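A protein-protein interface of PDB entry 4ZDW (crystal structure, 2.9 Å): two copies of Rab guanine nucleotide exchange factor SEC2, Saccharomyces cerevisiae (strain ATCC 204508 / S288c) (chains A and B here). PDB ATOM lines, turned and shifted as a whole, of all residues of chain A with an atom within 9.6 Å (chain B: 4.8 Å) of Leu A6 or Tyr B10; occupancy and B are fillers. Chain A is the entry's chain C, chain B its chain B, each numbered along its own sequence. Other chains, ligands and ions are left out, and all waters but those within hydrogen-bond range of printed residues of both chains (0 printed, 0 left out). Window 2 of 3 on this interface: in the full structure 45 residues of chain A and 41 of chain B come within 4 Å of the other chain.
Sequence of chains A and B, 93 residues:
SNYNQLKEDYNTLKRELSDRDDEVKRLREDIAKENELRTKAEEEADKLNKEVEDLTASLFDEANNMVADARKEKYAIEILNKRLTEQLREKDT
O of Lys A7 sits at hydrogen-bond distance from ND2 of Asn A11 (3.1 Å).
Of the 16 printed residues of chain A, 6 touch a printed residue of chain B. Hydrophobic or aromatic side chains of chain A that line the printed part of chain B: Leu A6, Tyr A10 and Leu A13. Along chain A the printed residues that touch a printed residue of chain B span positions 6 to 14. Printed residues of chain B that touch a printed residue of chain A: Leu B6, Asp B9, Tyr B10 and Leu B13. Hydrophobic or aromatic side chains of chain B within 4 Å of the printed part of chain A: Leu B6, Tyr B10 and Leu B13.
Among the printed residues, merely in contact across the chains: Leu A6 with Leu B6, Lys A14 with Leu B13, Leu A13 with Leu B13, Asp A9 with Tyr B10, Tyr A10 with Tyr B10, Tyr A10 with Leu B13, Tyr A10 with Asp B9, Leu A13 with Tyr B10, Lys A7 with Leu B6 and Leu A6 with Tyr B10.
Leu B6 touches its own counterpart, Leu A6. Lys A7 touches Leu B6, but with the chains exchanged Leu A6 does not touch Lys B7 (4.5 Å). Leu A13 touches its own counterpart, Leu B13. Lys A14 touches Leu B13, but with the chains exchanged Leu A13 does not touch Lys B14 (4.4 Å). Of the 10 pairs that touch across the chains among the printed residues, 7 have their exchanged pair printed and touching as well.
Ser A1 touches none of the printed residues of chain B. Tyr A3 touches none of the printed residues of chain B. Printed residues of chain B within 4 Å of Leu A6: Leu B6 (3.3 Å) and Tyr B10 (3.996 Å). Printed residues of chain B within 4 Å of Lys A7: Leu B6 (3.99 Å). Of the printed residues of chain B, Tyr A10 touches Asp B9, Tyr B10 and Leu B13. Of the printed residues of chain A, Leu B6 touches Leu A6 and Lys A7. Of chain A, only Tyr A10 (3.9 Å) comes within 4 Å of Asp B9. Of the printed residues of chain A, Tyr B10 touches Leu A6, Asp A9, Tyr A10 and Leu A13. No residue of chain A comes within 4 Å of Asn B11. Of the printed residues of chain A, Leu B13 touches Tyr A10, Leu A13 and Lys A14. The nearest printed residue of chain B that does not touch Leu A6 is Lys B7 (4.5 Å).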
ATOM      1  N   SER A   1      17.188  -2.096 -28.963  1.00  0.00           N
ATOM      2  CA  SER A   1      15.749  -2.521 -28.849  1.00  0.00           C
ATOM      3  C   SER A   1      15.669  -3.931 -28.257  1.00  0.00           C
ATOM      4  O   SER A   1      15.104  -4.132 -27.182  1.00  0.00           O
ATOM      5  CB  SER A   1      15.028  -2.446 -30.203  1.00  0.00           C
ATOM      6  N   ASN A   2      16.237  -4.906 -28.957  1.00  0.00           N
ATOM      7  CA  ASN A   2      16.498  -6.181 -28.336  1.00  0.00           C
ATOM      8  C   ASN A   2      17.742  -6.103 -27.496  1.00  0.00           C
ATOM      9  O   ASN A   2      17.774  -6.641 -26.403  1.00  0.00           O
ATOM     10  CB  ASN A   2      16.622  -7.286 -29.362  1.00  0.00           C
ATOM     11  CG  ASN A   2      15.294  -7.941 -29.646  1.00  0.00           C
ATOM     12  OD1 ASN A   2      14.240  -7.276 -29.624  1.00  0.00           O
ATOM     13  ND2 ASN A   2      15.327  -9.257 -29.907  1.00  0.00           N
ATOM     14  N   TYR A   3      18.765  -5.417 -27.988  1.00  0.00           N
ATOM     15  CA  TYR A   3      19.935  -5.206 -27.172  1.00  0.00           C
ATOM     16  C   TYR A   3      19.508  -4.490 -25.907  1.00  0.00           C
ATOM     17  O   TYR A   3      19.981  -4.817 -24.835  1.00  0.00           O
ATOM     18  CB  TYR A   3      20.991  -4.383 -27.902  1.00  0.00           C
ATOM     19  CG  TYR A   3      22.267  -4.163 -27.077  1.00  0.00           C
ATOM     20  CD1 TYR A   3      23.274  -5.112 -27.083  1.00  0.00           C
ATOM     21  CD2 TYR A   3      22.488  -2.990 -26.379  1.00  0.00           C
ATOM     22  CE1 TYR A   3      24.490  -4.882 -26.446  1.00  0.00           C
ATOM     23  CE2 TYR A   3      23.665  -2.769 -25.668  1.00  0.00           C
ATOM     24  CZ  TYR A   3      24.687  -3.702 -25.747  1.00  0.00           C
ATOM     25  OH  TYR A   3      25.878  -3.524 -25.078  1.00  0.00           O
ATOM     26  N   ASN A   4      18.614  -3.515 -26.013  1.00  0.00           N
ATOM     27  CA  ASN A   4      18.192  -2.794 -24.820  1.00  0.00           C
ATOM     28  C   ASN A   4      17.330  -3.660 -23.928  1.00  0.00           C
ATOM     29  O   ASN A   4      17.431  -3.618 -22.709  1.00  0.00           O
ATOM     30  CB  ASN A   4      17.449  -1.517 -25.179  1.00  0.00           C
ATOM     31  CG  ASN A   4      18.341  -0.483 -25.855  1.00  0.00           C
ATOM     32  OD1 ASN A   4      19.567  -0.516 -25.745  1.00  0.00           O
ATOM     33  ND2 ASN A   4      17.717   0.457 -26.546  1.00  0.00           N
ATOM     34  N   GLN A   5      16.488  -4.472 -24.541  1.00  0.00           N
ATOM     35  CA  GLN A   5      15.544  -5.249 -23.769  1.00  0.00           C
ATOM     36  C   GLN A   5      16.275  -6.242 -22.912  1.00  0.00           C
ATOM     37  O   GLN A   5      15.889  -6.500 -21.773  1.00  0.00           O
ATOM     38  CB  GLN A   5      14.548  -5.968 -24.676  1.00  0.00           C
ATOM     39  CG  GLN A   5      13.258  -6.337 -23.965  1.00  0.00           C
ATOM     40  CD  GLN A   5      12.814  -5.261 -22.973  1.00  0.00           C
ATOM     41  OE1 GLN A   5      13.121  -4.071 -23.133  1.00  0.00           O
ATOM     42  NE2 GLN A   5      12.085  -5.673 -21.943  1.00  0.00           N
ATOM     43  N   LEU A   6      17.330  -6.793 -23.495  1.00  0.00           N
ATOM     44  CA  LEU A   6      18.206  -7.734 -22.843  1.00  0.00           C
ATOM     45  C   LEU A   6      18.873  -7.048 -21.674  1.00  0.00           C
ATOM     46  O   LEU A   6      18.813  -7.533 -20.571  1.00  0.00           O
ATOM     47  CB  LEU A   6      19.264  -8.180 -23.824  1.00  0.00           C
ATOM     48  CG  LEU A   6      20.101  -9.335 -23.348  1.00  0.00           C
ATOM     49  CD1 LEU A   6      19.408 -10.585 -23.840  1.00  0.00           C
ATOM     50  CD2 LEU A   6      21.516  -9.269 -23.884  1.00  0.00           C
ATOM     51  N   LYS A   7      19.481  -5.893 -21.921  1.00  0.00           N
ATOM     52  CA  LYS A   7      20.154  -5.115 -20.879  1.00  0.00           C
ATOM     53  C   LYS A   7      19.343  -4.977 -19.603  1.00  0.00           C
ATOM     54  O   LYS A   7      19.880  -5.102 -18.497  1.00  0.00           O
ATOM     55  CB  LYS A   7      20.488  -3.724 -21.397  1.00  0.00           C
ATOM     56  CG  LYS A   7      21.781  -3.656 -22.182  1.00  0.00           C
ATOM     57  CD  LYS A   7      22.996  -3.864 -21.275  1.00  0.00           C
ATOM     58  CE  LYS A   7      24.204  -3.100 -21.825  1.00  0.00           C
ATOM     59  NZ  LYS A   7      23.974  -1.616 -21.965  1.00  0.00           N
ATOM     60  N   GLU A   8      18.052  -4.718 -19.748  1.00  0.00           N
ATOM     61  CA  GLU A   8      17.250  -4.499 -18.583  1.00  0.00           C
ATOM     62  C   GLU A   8      16.613  -5.765 -18.073  1.00  0.00           C
ATOM     63  O   GLU A   8      16.193  -5.821 -16.921  1.00  0.00           O
ATOM     64  CB  GLU A   8      16.216  -3.434 -18.842  1.00  0.00           C
ATOM     65  CG  GLU A   8      15.183  -3.802 -19.881  1.00  0.00           C
ATOM     66  CD  GLU A   8      13.929  -2.971 -19.697  1.00  0.00           C
ATOM     67  OE1 GLU A   8      13.159  -3.279 -18.757  1.00  0.00           O
ATOM     68  OE2 GLU A   8      13.718  -2.003 -20.471  1.00  0.00           O
ATOM     69  N   ASP A   9      16.523  -6.791 -18.913  1.00  0.00           N
ATOM     70  CA  ASP A   9      16.047  -8.077 -18.415  1.00  0.00           C
ATOM     71  C   ASP A   9      17.094  -8.626 -17.527  1.00  0.00           C
ATOM     72  O   ASP A   9      16.788  -9.157 -16.474  1.00  0.00           O
ATOM     73  CB  ASP A   9      15.735  -9.054 -19.515  1.00  0.00           C
ATOM     74  CG  ASP A   9      14.431  -8.748 -20.181  1.00  0.00           C
ATOM     75  OD1 ASP A   9      13.706  -7.860 -19.706  1.00  0.00           O
ATOM     76  OD2 ASP A   9      14.124  -9.389 -21.189  1.00  0.00           O
ATOM     77  N   TYR A  10      18.339  -8.459 -17.938  1.00  0.00           N
ATOM     78  CA  TYR A  10      19.451  -8.719 -17.069  1.00  0.00           C
ATOM     79  C   TYR A  10      19.246  -7.966 -15.781  1.00  0.00           C
ATOM     80  O   TYR A  10      19.166  -8.582 -14.751  1.00  0.00           O
ATOM     81  CB  TYR A  10      20.754  -8.303 -17.713  1.00  0.00           C
ATOM     82  CG  TYR A  10      21.963  -8.848 -17.000  1.00  0.00           C
ATOM     83  CD1 TYR A  10      22.653  -8.073 -16.074  1.00  0.00           C
ATOM     84  CD2 TYR A  10      22.422 -10.136 -17.252  1.00  0.00           C
ATOM     85  CE1 TYR A  10      23.767  -8.562 -15.416  1.00  0.00           C
ATOM     86  CE2 TYR A  10      23.534 -10.639 -16.596  1.00  0.00           C
ATOM     87  CZ  TYR A  10      24.205  -9.846 -15.675  1.00  0.00           C
ATOM     88  OH  TYR A  10      25.320 -10.326 -15.006  1.00  0.00           O
ATOM     89  N   ASN A  11      19.109  -6.651 -15.820  1.00  0.00           N
ATOM     90  CA  ASN A  11      18.953  -5.909 -14.576  1.00  0.00           C
ATOM     91  C   ASN A  11      17.844  -6.409 -13.679  1.00  0.00           C
ATOM     92  O   ASN A  11      18.030  -6.503 -12.472  1.00  0.00           O
ATOM     93  CB  ASN A  11      18.782  -4.435 -14.842  1.00  0.00           C
ATOM     94  CG  ASN A  11      20.038  -3.816 -15.403  1.00  0.00           C
ATOM     95  OD1 ASN A  11      21.150  -4.160 -14.995  1.00  0.00           O
ATOM     96  ND2 ASN A  11      19.873  -2.894 -16.344  1.00  0.00           N
ATOM     97  N   THR A  12      16.702  -6.748 -14.264  1.00  0.00           N
ATOM     98  CA  THR A  12      15.579  -7.279 -13.502  1.00  0.00           C
ATOM     99  C   THR A  12      15.979  -8.543 -12.741  1.00  0.00           C
ATOM    100  O   THR A  12      15.844  -8.622 -11.511  1.00  0.00           O
ATOM    101  CB  THR A  12      14.401  -7.602 -14.426  1.00  0.00           C
ATOM    102  OG1 THR A  12      14.094  -6.446 -15.201  1.00  0.00           O
ATOM    103  CG2 THR A  12      13.180  -8.033 -13.632  1.00  0.00           C
ATOM    104  N   LEU A  13      16.471  -9.533 -13.479  1.00  0.00           N
ATOM    105  CA  LEU A  13      16.825 -10.802 -12.882  1.00  0.00           C
ATOM    106  C   LEU A  13      18.013 -10.621 -11.969  1.00  0.00           C
ATOM    107  O   LEU A  13      18.069 -11.231 -10.925  1.00  0.00           O
ATOM    108  CB  LEU A  13      17.047 -11.872 -13.943  1.00  0.00           C
ATOM    109  CG  LEU A  13      15.773 -12.083 -14.781  1.00  0.00           C
ATOM    110  CD1 LEU A  13      15.904 -13.227 -15.758  1.00  0.00           C
ATOM    111  CD2 LEU A  13      14.528 -12.309 -13.933  1.00  0.00           C
ATOM    112  N   LYS A  14      18.922  -9.723 -12.305  1.00  0.00           N
ATOM    113  CA  LYS A  14      19.972  -9.354 -11.377  1.00  0.00           C
ATOM    114  C   LYS A  14      19.446  -9.104  -9.950  1.00  0.00           C
ATOM    115  O   LYS A  14      20.017  -9.626  -8.966  1.00  0.00           O
ATOM    116  CB  LYS A  14      20.745  -8.144 -11.887  1.00  0.00           C
ATOM    117  CG  LYS A  14      22.030  -7.862 -11.134  1.00  0.00           C
ATOM    118  CD  LYS A  14      22.796  -9.135 -10.777  1.00  0.00           C
ATOM    119  CE  LYS A  14      23.980  -8.816  -9.876  1.00  0.00           C
ATOM    120  NZ  LYS A  14      24.797  -7.718 -10.497  1.00  0.00           N
ATOM    121  N   GLU A  16      16.139  -9.856  -9.036  1.00  0.00           N
ATOM    122  CA  GLU A  16      15.369 -11.063  -8.715  1.00  0.00           C
ATOM    123  C   GLU A  16      16.219 -12.078  -8.031  1.00  0.00           C
ATOM    124  O   GLU A  16      15.729 -12.795  -7.191  1.00  0.00           O
ATOM    125  CB  GLU A  16      14.749 -11.709  -9.935  1.00  0.00           C
ATOM    126  CG  GLU A  16      13.302 -11.347 -10.130  1.00  0.00           C
ATOM    127  CD  GLU A  16      12.491 -11.620  -8.899  1.00  0.00           C
ATOM    128  OE1 GLU A  16      12.327 -10.695  -8.086  1.00  0.00           O
ATOM    129  OE2 GLU A  16      12.034 -12.758  -8.727  1.00  0.00           O
ATOM    130  N   LEU A  17      17.496 -12.126  -8.402  1.00  0.00           N
ATOM    131  CA  LEU A  17      18.482 -13.008  -7.770  1.00  0.00           C
ATOM    132  C   LEU A  17      18.900 -12.487  -6.418  1.00  0.00           C
ATOM    133  O   LEU A  17      18.801 -13.192  -5.434  1.00  0.00           O
ATOM    134  CB  LEU A  17      19.741 -13.162  -8.628  1.00  0.00           C
ATOM    135  CG  LEU A  17      20.836 -14.015  -7.988  1.00  0.00           C
ATOM    136  CD1 LEU A  17      20.356 -15.445  -7.891  1.00  0.00           C
ATOM    137  CD2 LEU A  17      22.131 -13.969  -8.772  1.00  0.00           C
ATOM    138  N   LEU B   6      27.653 -10.529 -23.037  1.00  0.00           N
ATOM    139  CA  LEU B   6      26.306 -10.314 -22.554  1.00  0.00           C
ATOM    140  C   LEU B   6      25.440 -11.561 -22.658  1.00  0.00           C
ATOM    141  O   LEU B   6      25.080 -12.154 -21.633  1.00  0.00           O
ATOM    142  CB  LEU B   6      25.644  -9.156 -23.289  1.00  0.00           C
ATOM    143  CG  LEU B   6      24.547  -8.486 -22.463  1.00  0.00           C
ATOM    144  CD1 LEU B   6      25.105  -8.193 -21.066  1.00  0.00           C
ATOM    145  CD2 LEU B   6      24.038  -7.229 -23.153  1.00  0.00           C
ATOM    146  N   LYS B   7      25.127 -11.961 -23.891  1.00  0.00           N
ATOM    147  CA  LYS B   7      24.214 -13.074 -24.151  1.00  0.00           C
ATOM    148  C   LYS B   7      24.538 -14.233 -23.225  1.00  0.00           C
ATOM    149  O   LYS B   7      23.644 -14.888 -22.683  1.00  0.00           O
ATOM    150  CB  LYS B   7      24.268 -13.494 -25.626  1.00  0.00           C
ATOM    151  CG  LYS B   7      23.261 -14.564 -26.044  1.00  0.00           C
ATOM    152  CD  LYS B   7      21.817 -14.240 -25.638  1.00  0.00           C
ATOM    153  CE  LYS B   7      20.771 -15.143 -26.322  1.00  0.00           C
ATOM    154  NZ  LYS B   7      20.413 -16.432 -25.639  1.00  0.00           N
ATOM    155  N   GLU B   8      25.830 -14.423 -22.996  1.00  0.00           N
ATOM    156  CA  GLU B   8      26.329 -15.502 -22.177  1.00  0.00           C
ATOM    157  C   GLU B   8      26.190 -15.214 -20.702  1.00  0.00           C
ATOM    158  O   GLU B   8      25.868 -16.113 -19.939  1.00  0.00           O
ATOM    159  CB  GLU B   8      27.786 -15.727 -22.485  1.00  0.00           C
ATOM    160  CG  GLU B   8      28.152 -17.183 -22.605  1.00  0.00           C
ATOM    161  CD  GLU B   8      29.646 -17.386 -22.528  1.00  0.00           C
ATOM    162  OE1 GLU B   8      30.343 -17.073 -23.527  1.00  0.00           O
ATOM    163  OE2 GLU B   8      30.116 -17.854 -21.461  1.00  0.00           O
ATOM    164  N   ASP B   9      26.446 -13.978 -20.285  1.00  0.00           N
ATOM    165  CA  ASP B   9      26.309 -13.668 -18.871  1.00  0.00           C
ATOM    166  C   ASP B   9      24.887 -13.795 -18.403  1.00  0.00           C
ATOM    167  O   ASP B   9      24.630 -14.358 -17.333  1.00  0.00           O
ATOM    168  CB  ASP B   9      26.815 -12.281 -18.541  1.00  0.00           C
ATOM    169  CG  ASP B   9      28.320 -12.224 -18.428  1.00  0.00           C
ATOM    170  OD1 ASP B   9      28.965 -13.273 -18.198  1.00  0.00           O
ATOM    171  OD2 ASP B   9      28.857 -11.105 -18.585  1.00  0.00           O
ATOM    172  N   TYR B  10      23.969 -13.275 -19.212  1.00  0.00           N
ATOM    173  CA  TYR B  10      22.551 -13.413 -18.954  1.00  0.00           C
ATOM    174  C   TYR B  10      22.151 -14.872 -18.801  1.00  0.00           C
ATOM    175  O   TYR B  10      21.542 -15.259 -17.801  1.00  0.00           O
ATOM    176  CB  TYR B  10      21.791 -12.782 -20.076  1.00  0.00           C
ATOM    177  CG  TYR B  10      20.294 -12.749 -19.911  1.00  0.00           C
ATOM    178  CD1 TYR B  10      19.699 -12.142 -18.823  1.00  0.00           C
ATOM    179  CD2 TYR B  10      19.468 -13.288 -20.898  1.00  0.00           C
ATOM    180  CE1 TYR B  10      18.322 -12.099 -18.702  1.00  0.00           C
ATOM    181  CE2 TYR B  10      18.097 -13.244 -20.800  1.00  0.00           C
ATOM    182  CZ  TYR B  10      17.517 -12.651 -19.701  1.00  0.00           C
ATOM    183  OH  TYR B  10      16.128 -12.611 -19.626  1.00  0.00           O
ATOM    184  N   ASN B  11      22.512 -15.699 -19.772  1.00  0.00           N
ATOM    185  CA  ASN B  11      22.367 -17.141 -19.582  1.00  0.00           C
ATOM    186  C   ASN B  11      22.970 -17.711 -18.290  1.00  0.00           C
ATOM    187  O   ASN B  11      22.392 -18.611 -17.705  1.00  0.00           O
ATOM    188  CB  ASN B  11      22.851 -17.894 -20.808  1.00  0.00           C
ATOM    189  CG  ASN B  11      21.856 -17.817 -21.947  1.00  0.00           C
ATOM    190  OD1 ASN B  11      20.686 -18.103 -21.766  1.00  0.00           O
ATOM    191  ND2 ASN B  11      22.308 -17.418 -23.106  1.00  0.00           N
ATOM    192  N   THR B  12      24.095 -17.179 -17.821  1.00  0.00           N
ATOM    193  CA  THR B  12      24.667 -17.665 -16.572  1.00  0.00           C
ATOM    194  C   THR B  12      23.782 -17.210 -15.441  1.00  0.00           C
ATOM    195  O   THR B  12      23.369 -18.011 -14.597  1.00  0.00           O
ATOM    196  CB  THR B  12      26.088 -17.140 -16.315  1.00  0.00           C
ATOM    197  OG1 THR B  12      26.968 -17.585 -17.350  1.00  0.00           O
ATOM    198  CG2 THR B  12      26.623 -17.649 -14.988  1.00  0.00           C
ATOM    199  N   LEU B  13      23.484 -15.917 -15.432  1.00  0.00           N
ATOM    200  CA  LEU B  13      22.571 -15.351 -14.441  1.00  0.00           C
ATOM    201  C   LEU B  13      21.251 -16.094 -14.368  1.00  0.00           C
ATOM    202  O   LEU B  13      20.793 -16.370 -13.279  1.00  0.00           O
ATOM    203  CB  LEU B  13      22.294 -13.879 -14.719  1.00  0.00           C
ATOM    204  CG  LEU B  13      21.423 -13.217 -13.662  1.00  0.00           C
ATOM    205  CD1 LEU B  13      22.341 -12.709 -12.563  1.00  0.00           C
ATOM    206  CD2 LEU B  13      20.591 -12.079 -14.227  1.00  0.00           C
ATOM    207  N   LYS B  14      20.649 -16.418 -15.512  1.00  0.00           N
ATOM    208  CA  LYS B  14      19.438 -17.225 -15.541  1.00  0.00           C
ATOM    209  C   LYS B  14      19.512 -18.540 -14.754  1.00  0.00           C
ATOM    210  O   LYS B  14      18.570 -18.935 -14.052  1.00  0.00           O
ATOM    211  CB  LYS B  14      19.076 -17.528 -16.964  1.00  0.00           C
ATOM    212  CG  LYS B  14      18.145 -16.505 -17.535  1.00  0.00           C
ATOM    213  CD  LYS B  14      18.343 -16.353 -19.024  1.00  0.00           C
ATOM    214  CE  LYS B  14      17.407 -17.272 -19.766  1.00  0.00           C
ATOM    215  NZ  LYS B  14      17.640 -17.138 -21.227  1.00  0.00           N
